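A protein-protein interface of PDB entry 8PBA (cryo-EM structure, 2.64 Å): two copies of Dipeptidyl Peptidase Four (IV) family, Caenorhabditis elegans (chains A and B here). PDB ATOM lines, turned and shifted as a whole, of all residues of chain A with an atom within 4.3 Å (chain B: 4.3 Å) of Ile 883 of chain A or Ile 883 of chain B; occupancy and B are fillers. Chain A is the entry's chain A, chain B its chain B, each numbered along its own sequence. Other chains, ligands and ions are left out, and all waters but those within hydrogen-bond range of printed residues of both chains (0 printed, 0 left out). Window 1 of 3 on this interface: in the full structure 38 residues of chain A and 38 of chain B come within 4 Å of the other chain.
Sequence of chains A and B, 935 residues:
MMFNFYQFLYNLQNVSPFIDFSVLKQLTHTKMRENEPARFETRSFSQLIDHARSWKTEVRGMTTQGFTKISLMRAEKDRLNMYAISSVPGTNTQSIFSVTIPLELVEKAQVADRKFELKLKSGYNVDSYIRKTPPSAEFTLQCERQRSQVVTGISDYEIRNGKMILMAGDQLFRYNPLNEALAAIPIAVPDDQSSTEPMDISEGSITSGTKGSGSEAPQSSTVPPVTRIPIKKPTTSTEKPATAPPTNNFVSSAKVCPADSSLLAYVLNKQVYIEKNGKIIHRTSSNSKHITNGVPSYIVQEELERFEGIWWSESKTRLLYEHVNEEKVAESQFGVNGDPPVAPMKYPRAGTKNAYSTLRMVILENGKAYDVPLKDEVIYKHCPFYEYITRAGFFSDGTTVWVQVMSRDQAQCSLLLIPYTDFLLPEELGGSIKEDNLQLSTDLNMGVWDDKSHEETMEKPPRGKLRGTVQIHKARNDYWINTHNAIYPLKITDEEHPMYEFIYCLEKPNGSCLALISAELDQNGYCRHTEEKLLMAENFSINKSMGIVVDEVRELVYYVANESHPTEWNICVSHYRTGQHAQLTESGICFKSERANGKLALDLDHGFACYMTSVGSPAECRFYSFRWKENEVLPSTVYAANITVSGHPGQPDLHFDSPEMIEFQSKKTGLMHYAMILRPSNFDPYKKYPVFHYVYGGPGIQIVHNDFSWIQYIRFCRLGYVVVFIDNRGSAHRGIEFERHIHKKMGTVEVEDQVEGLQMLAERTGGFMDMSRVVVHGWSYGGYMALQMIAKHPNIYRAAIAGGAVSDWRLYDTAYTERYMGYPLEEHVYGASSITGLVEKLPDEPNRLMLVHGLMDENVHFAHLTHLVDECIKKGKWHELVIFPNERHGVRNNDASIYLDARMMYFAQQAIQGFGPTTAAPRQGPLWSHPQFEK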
ATOM      1  N   HIS A 853     -21.962  11.895   2.371  1.00  0.00           N
ATOM      2  CA  HIS A 853     -20.610  11.758   2.868  1.00  0.00           C
ATOM      3  C   HIS A 853     -20.156  12.963   3.669  1.00  0.00           C
ATOM      4  O   HIS A 853     -20.510  14.102   3.360  1.00  0.00           O
ATOM      5  CB  HIS A 853     -19.683  11.557   1.686  1.00  0.00           C
ATOM      6  CG  HIS A 853     -18.528  10.704   1.959  1.00  0.00           C
ATOM      7  ND1 HIS A 853     -17.492  11.107   2.716  1.00  0.00           N
ATOM      8  CD2 HIS A 853     -18.228   9.460   1.542  1.00  0.00           C
ATOM      9  CE1 HIS A 853     -16.601  10.158   2.776  1.00  0.00           C
ATOM     10  NE2 HIS A 853     -17.025   9.142   2.073  1.00  0.00           N
ATOM     11  N   LEU A 855     -17.155  15.546   4.862  1.00  0.00           N
ATOM     12  CA  LEU A 855     -15.990  16.080   4.181  1.00  0.00           C
ATOM     13  C   LEU A 855     -14.722  15.829   4.988  1.00  0.00           C
ATOM     14  O   LEU A 855     -13.619  15.839   4.446  1.00  0.00           O
ATOM     15  CB  LEU A 855     -16.189  17.574   3.931  1.00  0.00           C
ATOM     16  CG  LEU A 855     -15.176  18.293   3.024  1.00  0.00           C
ATOM     17  CD1 LEU A 855     -15.188  17.690   1.639  1.00  0.00           C
ATOM     18  CD2 LEU A 855     -15.537  19.765   2.961  1.00  0.00           C
ATOM     19  N   PHE A 862     -12.986  11.176   1.738  1.00  0.00           N
ATOM     20  CA  PHE A 862     -13.784  11.839   0.731  1.00  0.00           C
ATOM     21  C   PHE A 862     -13.315  11.422  -0.647  1.00  0.00           C
ATOM     22  O   PHE A 862     -14.116  11.294  -1.569  1.00  0.00           O
ATOM     23  CB  PHE A 862     -13.676  13.334   0.900  1.00  0.00           C
ATOM     24  CG  PHE A 862     -14.686  14.089   0.183  1.00  0.00           C
ATOM     25  CD1 PHE A 862     -15.974  14.095   0.617  1.00  0.00           C
ATOM     26  CD2 PHE A 862     -14.352  14.832  -0.904  1.00  0.00           C
ATOM     27  CE1 PHE A 862     -16.907  14.823  -0.028  1.00  0.00           C
ATOM     28  CE2 PHE A 862     -15.287  15.559  -1.557  1.00  0.00           C
ATOM     29  CZ  PHE A 862     -16.563  15.553  -1.124  1.00  0.00           C
ATOM     30  N   VAL A 869     -18.171   9.717  -7.753  1.00  0.00           N
ATOM     31  CA  VAL A 869     -18.861  10.787  -8.445  1.00  0.00           C
ATOM     32  C   VAL A 869     -18.261  10.997  -9.816  1.00  0.00           C
ATOM     33  O   VAL A 869     -18.983  11.199 -10.789  1.00  0.00           O
ATOM     34  CB  VAL A 869     -18.810  12.087  -7.629  1.00  0.00           C
ATOM     35  CG1 VAL A 869     -19.276  13.256  -8.462  1.00  0.00           C
ATOM     36  CG2 VAL A 869     -19.703  11.940  -6.412  1.00  0.00           C
ATOM     37  N   ILE A 873     -20.100  10.726 -13.542  1.00  0.00           N
ATOM     38  CA  ILE A 873     -20.094  11.798 -14.520  1.00  0.00           C
ATOM     39  C   ILE A 873     -19.683  11.264 -15.876  1.00  0.00           C
ATOM     40  O   ILE A 873     -20.311  11.563 -16.890  1.00  0.00           O
ATOM     41  CB  ILE A 873     -19.151  12.930 -14.085  1.00  0.00           C
ATOM     42  CG1 ILE A 873     -19.717  13.639 -12.857  1.00  0.00           C
ATOM     43  CG2 ILE A 873     -18.942  13.901 -15.216  1.00  0.00           C
ATOM     44  CD1 ILE A 873     -18.744  14.553 -12.158  1.00  0.00           C
ATOM     45  N   LEU A 881     -26.403  14.096  -4.216  1.00  0.00           N
ATOM     46  CA  LEU A 881     -25.276  14.171  -3.304  1.00  0.00           C
ATOM     47  C   LEU A 881     -25.504  15.114  -2.137  1.00  0.00           C
ATOM     48  O   LEU A 881     -25.840  16.281  -2.319  1.00  0.00           O
ATOM     49  CB  LEU A 881     -24.033  14.584  -4.086  1.00  0.00           C
ATOM     50  CG  LEU A 881     -22.817  14.918  -3.282  1.00  0.00           C
ATOM     51  CD1 LEU A 881     -22.363  13.706  -2.513  1.00  0.00           C
ATOM     52  CD2 LEU A 881     -21.738  15.395  -4.230  1.00  0.00           C
ATOM     53  N   VAL A 882     -25.283  14.600  -0.933  1.00  0.00           N
ATOM     54  CA  VAL A 882     -25.363  15.401   0.277  1.00  0.00           C
ATOM     55  C   VAL A 882     -24.035  15.371   1.016  1.00  0.00           C
ATOM     56  O   VAL A 882     -23.479  14.303   1.264  1.00  0.00           O
ATOM     57  CB  VAL A 882     -26.478  14.884   1.196  1.00  0.00           C
ATOM     58  CG1 VAL A 882     -26.550  15.704   2.465  1.00  0.00           C
ATOM     59  CG2 VAL A 882     -27.787  14.935   0.469  1.00  0.00           C
ATOM     60  N   ILE A 883     -23.505  16.547   1.308  1.00  0.00           N
ATOM     61  CA  ILE A 883     -22.228  16.666   1.990  1.00  0.00           C
ATOM     62  C   ILE A 883     -22.331  17.460   3.264  1.00  0.00           C
ATOM     63  O   ILE A 883     -23.045  18.457   3.332  1.00  0.00           O
ATOM     64  CB  ILE A 883     -21.147  17.263   1.081  1.00  0.00           C
ATOM     65  CG1 ILE A 883     -20.861  16.288  -0.032  1.00  0.00           C
ATOM     66  CG2 ILE A 883     -19.870  17.589   1.877  1.00  0.00           C
ATOM     67  CD1 ILE A 883     -19.978  16.826  -1.091  1.00  0.00           C
ATOM     68  N   PHE A 884     -21.609  16.998   4.272  1.00  0.00           N
ATOM     69  CA  PHE A 884     -21.529  17.659   5.563  1.00  0.00           C
ATOM     70  C   PHE A 884     -20.107  18.134   5.841  1.00  0.00           C
ATOM     71  O   PHE A 884     -19.288  17.363   6.343  1.00  0.00           O
ATOM     72  CB  PHE A 884     -21.955  16.699   6.649  1.00  0.00           C
ATOM     73  CG  PHE A 884     -23.348  16.313   6.554  1.00  0.00           C
ATOM     74  CD1 PHE A 884     -23.742  15.337   5.698  1.00  0.00           C
ATOM     75  CD2 PHE A 884     -24.283  16.934   7.319  1.00  0.00           C
ATOM     76  CE1 PHE A 884     -25.050  15.011   5.583  1.00  0.00           C
ATOM     77  CE2 PHE A 884     -25.595  16.609   7.211  1.00  0.00           C
ATOM     78  CZ  PHE A 884     -25.976  15.653   6.325  1.00  0.00           C
ATOM     79  N   PRO A 885     -19.780  19.385   5.499  1.00  0.00           N
ATOM     80  CA  PRO A 885     -18.452  19.962   5.504  1.00  0.00           C
ATOM     81  C   PRO A 885     -17.765  19.927   6.855  1.00  0.00           C
ATOM     82  O   PRO A 885     -16.541  19.987   6.933  1.00  0.00           O
ATOM     83  CB  PRO A 885     -18.723  21.405   5.107  1.00  0.00           C
ATOM     84  CG  PRO A 885     -20.009  21.363   4.335  1.00  0.00           C
ATOM     85  CD  PRO A 885     -20.815  20.285   4.988  1.00  0.00           C
ATOM     86  N   HIS B 853     -20.557  23.090  -8.330  1.00  0.00           N
ATOM     87  CA  HIS B 853     -19.247  23.636  -8.048  1.00  0.00           C
ATOM     88  C   HIS B 853     -18.125  22.673  -8.388  1.00  0.00           C
ATOM     89  O   HIS B 853     -18.256  21.461  -8.222  1.00  0.00           O
ATOM     90  CB  HIS B 853     -19.181  23.990  -6.576  1.00  0.00           C
ATOM     91  CG  HIS B 853     -18.346  25.149  -6.267  1.00  0.00           C
ATOM     92  ND1 HIS B 853     -17.004  25.112  -6.328  1.00  0.00           N
ATOM     93  CD2 HIS B 853     -18.670  26.390  -5.857  1.00  0.00           C
ATOM     94  CE1 HIS B 853     -16.520  26.273  -5.987  1.00  0.00           C
ATOM     95  NE2 HIS B 853     -17.512  27.071  -5.698  1.00  0.00           N
ATOM     96  N   LEU B 855     -14.369  21.131  -7.606  1.00  0.00           N
ATOM     97  CA  LEU B 855     -13.644  20.887  -6.372  1.00  0.00           C
ATOM     98  C   LEU B 855     -12.270  21.545  -6.407  1.00  0.00           C
ATOM     99  O   LEU B 855     -11.667  21.798  -5.366  1.00  0.00           O
ATOM    100  CB  LEU B 855     -13.521  19.382  -6.144  1.00  0.00           C
ATOM    101  CG  LEU B 855     -12.986  18.901  -4.785  1.00  0.00           C
ATOM    102  CD1 LEU B 855     -13.893  19.363  -3.669  1.00  0.00           C
ATOM    103  CD2 LEU B 855     -12.901  17.386  -4.802  1.00  0.00           C
ATOM    104  N   PHE B 862     -13.881  26.218  -3.122  1.00  0.00           N
ATOM    105  CA  PHE B 862     -14.869  25.280  -2.636  1.00  0.00           C
ATOM    106  C   PHE B 862     -15.334  25.697  -1.256  1.00  0.00           C
ATOM    107  O   PHE B 862     -16.498  25.523  -0.910  1.00  0.00           O
ATOM    108  CB  PHE B 862     -14.278  23.893  -2.600  1.00  0.00           C
ATOM    109  CG  PHE B 862     -15.258  22.831  -2.465  1.00  0.00           C
ATOM    110  CD1 PHE B 862     -16.061  22.503  -3.510  1.00  0.00           C
ATOM    111  CD2 PHE B 862     -15.356  22.124  -1.309  1.00  0.00           C
ATOM    112  CE1 PHE B 862     -16.949  21.494  -3.397  1.00  0.00           C
ATOM    113  CE2 PHE B 862     -16.250  21.116  -1.190  1.00  0.00           C
ATOM    114  CZ  PHE B 862     -17.048  20.803  -2.230  1.00  0.00           C
ATOM    115  N   VAL B 869     -23.454  25.405   2.055  1.00  0.00           N
ATOM    116  CA  VAL B 869     -24.075  24.133   2.365  1.00  0.00           C
ATOM    117  C   VAL B 869     -24.258  23.987   3.857  1.00  0.00           C
ATOM    118  O   VAL B 869     -25.295  23.514   4.316  1.00  0.00           O
ATOM    119  CB  VAL B 869     -23.244  22.969   1.806  1.00  0.00           C
ATOM    120  CG1 VAL B 869     -23.733  21.652   2.360  1.00  0.00           C
ATOM    121  CG2 VAL B 869     -23.361  22.961   0.294  1.00  0.00           C
ATOM    122  N   ILE B 873     -27.775  23.434   6.017  1.00  0.00           N
ATOM    123  CA  ILE B 873     -27.989  22.330   6.932  1.00  0.00           C
ATOM    124  C   ILE B 873     -28.522  22.845   8.255  1.00  0.00           C
ATOM    125  O   ILE B 873     -29.478  22.303   8.806  1.00  0.00           O
ATOM    126  CB  ILE B 873     -26.688  21.542   7.154  1.00  0.00           C
ATOM    127  CG1 ILE B 873     -26.300  20.807   5.875  1.00  0.00           C
ATOM    128  CG2 ILE B 873     -26.847  20.579   8.301  1.00  0.00           C
ATOM    129  CD1 ILE B 873     -24.895  20.259   5.870  1.00  0.00           C
ATOM    130  N   LEU B 881     -26.983  19.215  -4.918  1.00  0.00           N
ATOM    131  CA  LEU B 881     -25.578  19.530  -5.089  1.00  0.00           C
ATOM    132  C   LEU B 881     -24.884  18.661  -6.121  1.00  0.00           C
ATOM    133  O   LEU B 881     -24.926  17.435  -6.050  1.00  0.00           O
ATOM    134  CB  LEU B 881     -24.876  19.417  -3.740  1.00  0.00           C
ATOM    135  CG  LEU B 881     -23.382  19.499  -3.753  1.00  0.00           C
ATOM    136  CD1 LEU B 881     -22.949  20.847  -4.262  1.00  0.00           C
ATOM    137  CD2 LEU B 881     -22.883  19.264  -2.343  1.00  0.00           C
ATOM    138  N   VAL B 882     -24.215  19.311  -7.065  1.00  0.00           N
ATOM    139  CA  VAL B 882     -23.419  18.620  -8.066  1.00  0.00           C
ATOM    140  C   VAL B 882     -21.972  19.076  -7.993  1.00  0.00           C
ATOM    141  O   VAL B 882     -21.690  20.274  -7.996  1.00  0.00           O
ATOM    142  CB  VAL B 882     -23.974  18.880  -9.474  1.00  0.00           C
ATOM    143  CG1 VAL B 882     -23.135  18.177 -10.517  1.00  0.00           C
ATOM    144  CG2 VAL B 882     -25.394  18.409  -9.543  1.00  0.00           C
ATOM    145  N   ILE B 883     -21.065  18.121  -7.866  1.00  0.00           N
ATOM    146  CA  ILE B 883     -19.648  18.417  -7.761  1.00  0.00           C
ATOM    147  C   ILE B 883     -18.837  17.733  -8.829  1.00  0.00           C
ATOM    148  O   ILE B 883     -19.099  16.586  -9.181  1.00  0.00           O
ATOM    149  CB  ILE B 883     -19.093  18.073  -6.373  1.00  0.00           C
ATOM    150  CG1 ILE B 883     -19.720  18.994  -5.361  1.00  0.00           C
ATOM    151  CG2 ILE B 883     -17.557  18.180  -6.348  1.00  0.00           C
ATOM    152  CD1 ILE B 883     -19.419  18.639  -3.955  1.00  0.00           C
ATOM    153  N   PHE B 884     -17.854  18.457  -9.337  1.00  0.00           N
ATOM    154  CA  PHE B 884     -16.927  17.951 -10.333  1.00  0.00           C
ATOM    155  C   PHE B 884     -15.505  17.913  -9.780  1.00  0.00           C
ATOM    156  O   PHE B 884     -14.797  18.919  -9.836  1.00  0.00           O
ATOM    157  CB  PHE B 884     -16.962  18.840 -11.554  1.00  0.00           C
ATOM    158  CG  PHE B 884     -18.238  18.815 -12.240  1.00  0.00           C
ATOM    159  CD1 PHE B 884     -19.277  19.572 -11.803  1.00  0.00           C
ATOM    160  CD2 PHE B 884     -18.413  18.024 -13.329  1.00  0.00           C
ATOM    161  CE1 PHE B 884     -20.478  19.511 -12.421  1.00  0.00           C
ATOM    162  CE2 PHE B 884     -19.615  17.962 -13.956  1.00  0.00           C
ATOM    163  CZ  PHE B 884     -20.653  18.699 -13.485  1.00  0.00           C
ATOM    164  N   PRO B 885     -15.076  16.779  -9.218  1.00  0.00           N
ATOM    165  CA  PRO B 885     -13.847  16.596  -8.474  1.00  0.00           C
ATOM    166  C   PRO B 885     -12.592  16.928  -9.258  1.00  0.00           C
ATOM    167  O   PRO B 885     -11.552  17.217  -8.674  1.00  0.00           O
ATOM    168  CB  PRO B 885     -13.873  15.107  -8.165  1.00  0.00           C
ATOM    169  CG  PRO B 885     -15.324  14.727  -8.192  1.00  0.00           C
ATOM    170  CD  PRO B 885     -15.927  15.588  -9.258  1.00  0.00           C
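Val 869 of chain A touches Ile 883 of chain B, and with the chains exchanged Ile 883 of chain A touches Val 869 of chain B.
Leu 881 of chain B touches its own counterpart, Leu 881 of chain A.
Leu 881 of chain A touches Ile 883 of chain B, and with the chains exchanged Ile 883 of chain A touches Leu 881 of chain B.
Ile 883 of chain A touches its own counterpart, Ile 883 of chain B.
Of the 10 pairs that touch across the chains among the printed residues, 10 have their exchanged pair printed and touching as well.
Of the 10 printed residues of chain B, 5 touch a printed residue of chain A.
Hydrophobic or aromatic side chains of chain B that line the printed part of chain A: Val 869, Ile 873, Leu 881, Ile 883 and Phe 884.
Of the 10 printed residues of chain A, 5 touch a printed residue of chain B.
Hydrophobic or aromatic side chains of chain A within 4 Å of the printed part of chain B: Val 869, Ile 873, Leu 881, Ile 883 and Phe 884.
Among the printed residues, 10 pairs touch across the chains.
Among the printed residues, no Asp or Glu carboxylate lies within 4 Å of a Lys or Arg side-chain nitrogen of the other chain.
N of Phe 884 of chain A lies within hydrogen-bond range of O of His 853 of chain A, at 3.2 Å.
The backbone NH (N) of Leu 855 of chain A sits at hydrogen-bond distance from the backbone carbonyl oxygen (O) of Phe 884 of chain A, at 3.2 Å.
The backbone carbonyl oxygen (O) of His 853 of chain B is in hydrogen-bond range of the backbone NH (N) of Phe 884 of chain B, at 3.2 Å.
O of Phe 884 of chain B lies within hydrogen-bond range of N of Leu 855 of chain B, at 3.2 Å.
Among the printed residues, pairs that only touch across the chains: Val 869 of chain A with Ile 883 of chain B, Ile 873 of chain A with Ile 883 of chain B, Ile 873 of chain A with Phe 884 of chain B, Leu 881 of chain A with Leu 881 of chain B, Leu 881 of chain A with Ile 883 of chain B, Ile 883 of chain A with Val 869 of chain B, Ile 883 of chain A with Ile 873 of chain B, Ile 883 of chain A with Leu 881 of chain B, Ile 883 of chain A with Ile 883 of chain B and Phe 884 of chain A with Ile 873 of chain B.
Printed residues of chain B within 4 Å of Ile 883 of chain A: Val 869, Ile 873, Leu 881 and Ile 883.
Of the printed residues of chain A, Ile 883 of chain B touches Val 869, Ile 873, Leu 881 and Ile 883.
Printed residues of chain B within 4 Å of Ile 873 of chain A: Ile 883 and Phe 884.
Of the printed residues of chain B, Leu 881 of chain A touches Leu 881 and Ile 883.
The nearest printed residue of chain A that does not touch Ile 883 of chain B is Phe 862 of chain A (5.1 Å).
The nearest printed residue of chain B that does not touch Leu 881 of chain A is Val 882 of chain B (5.3 Å).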
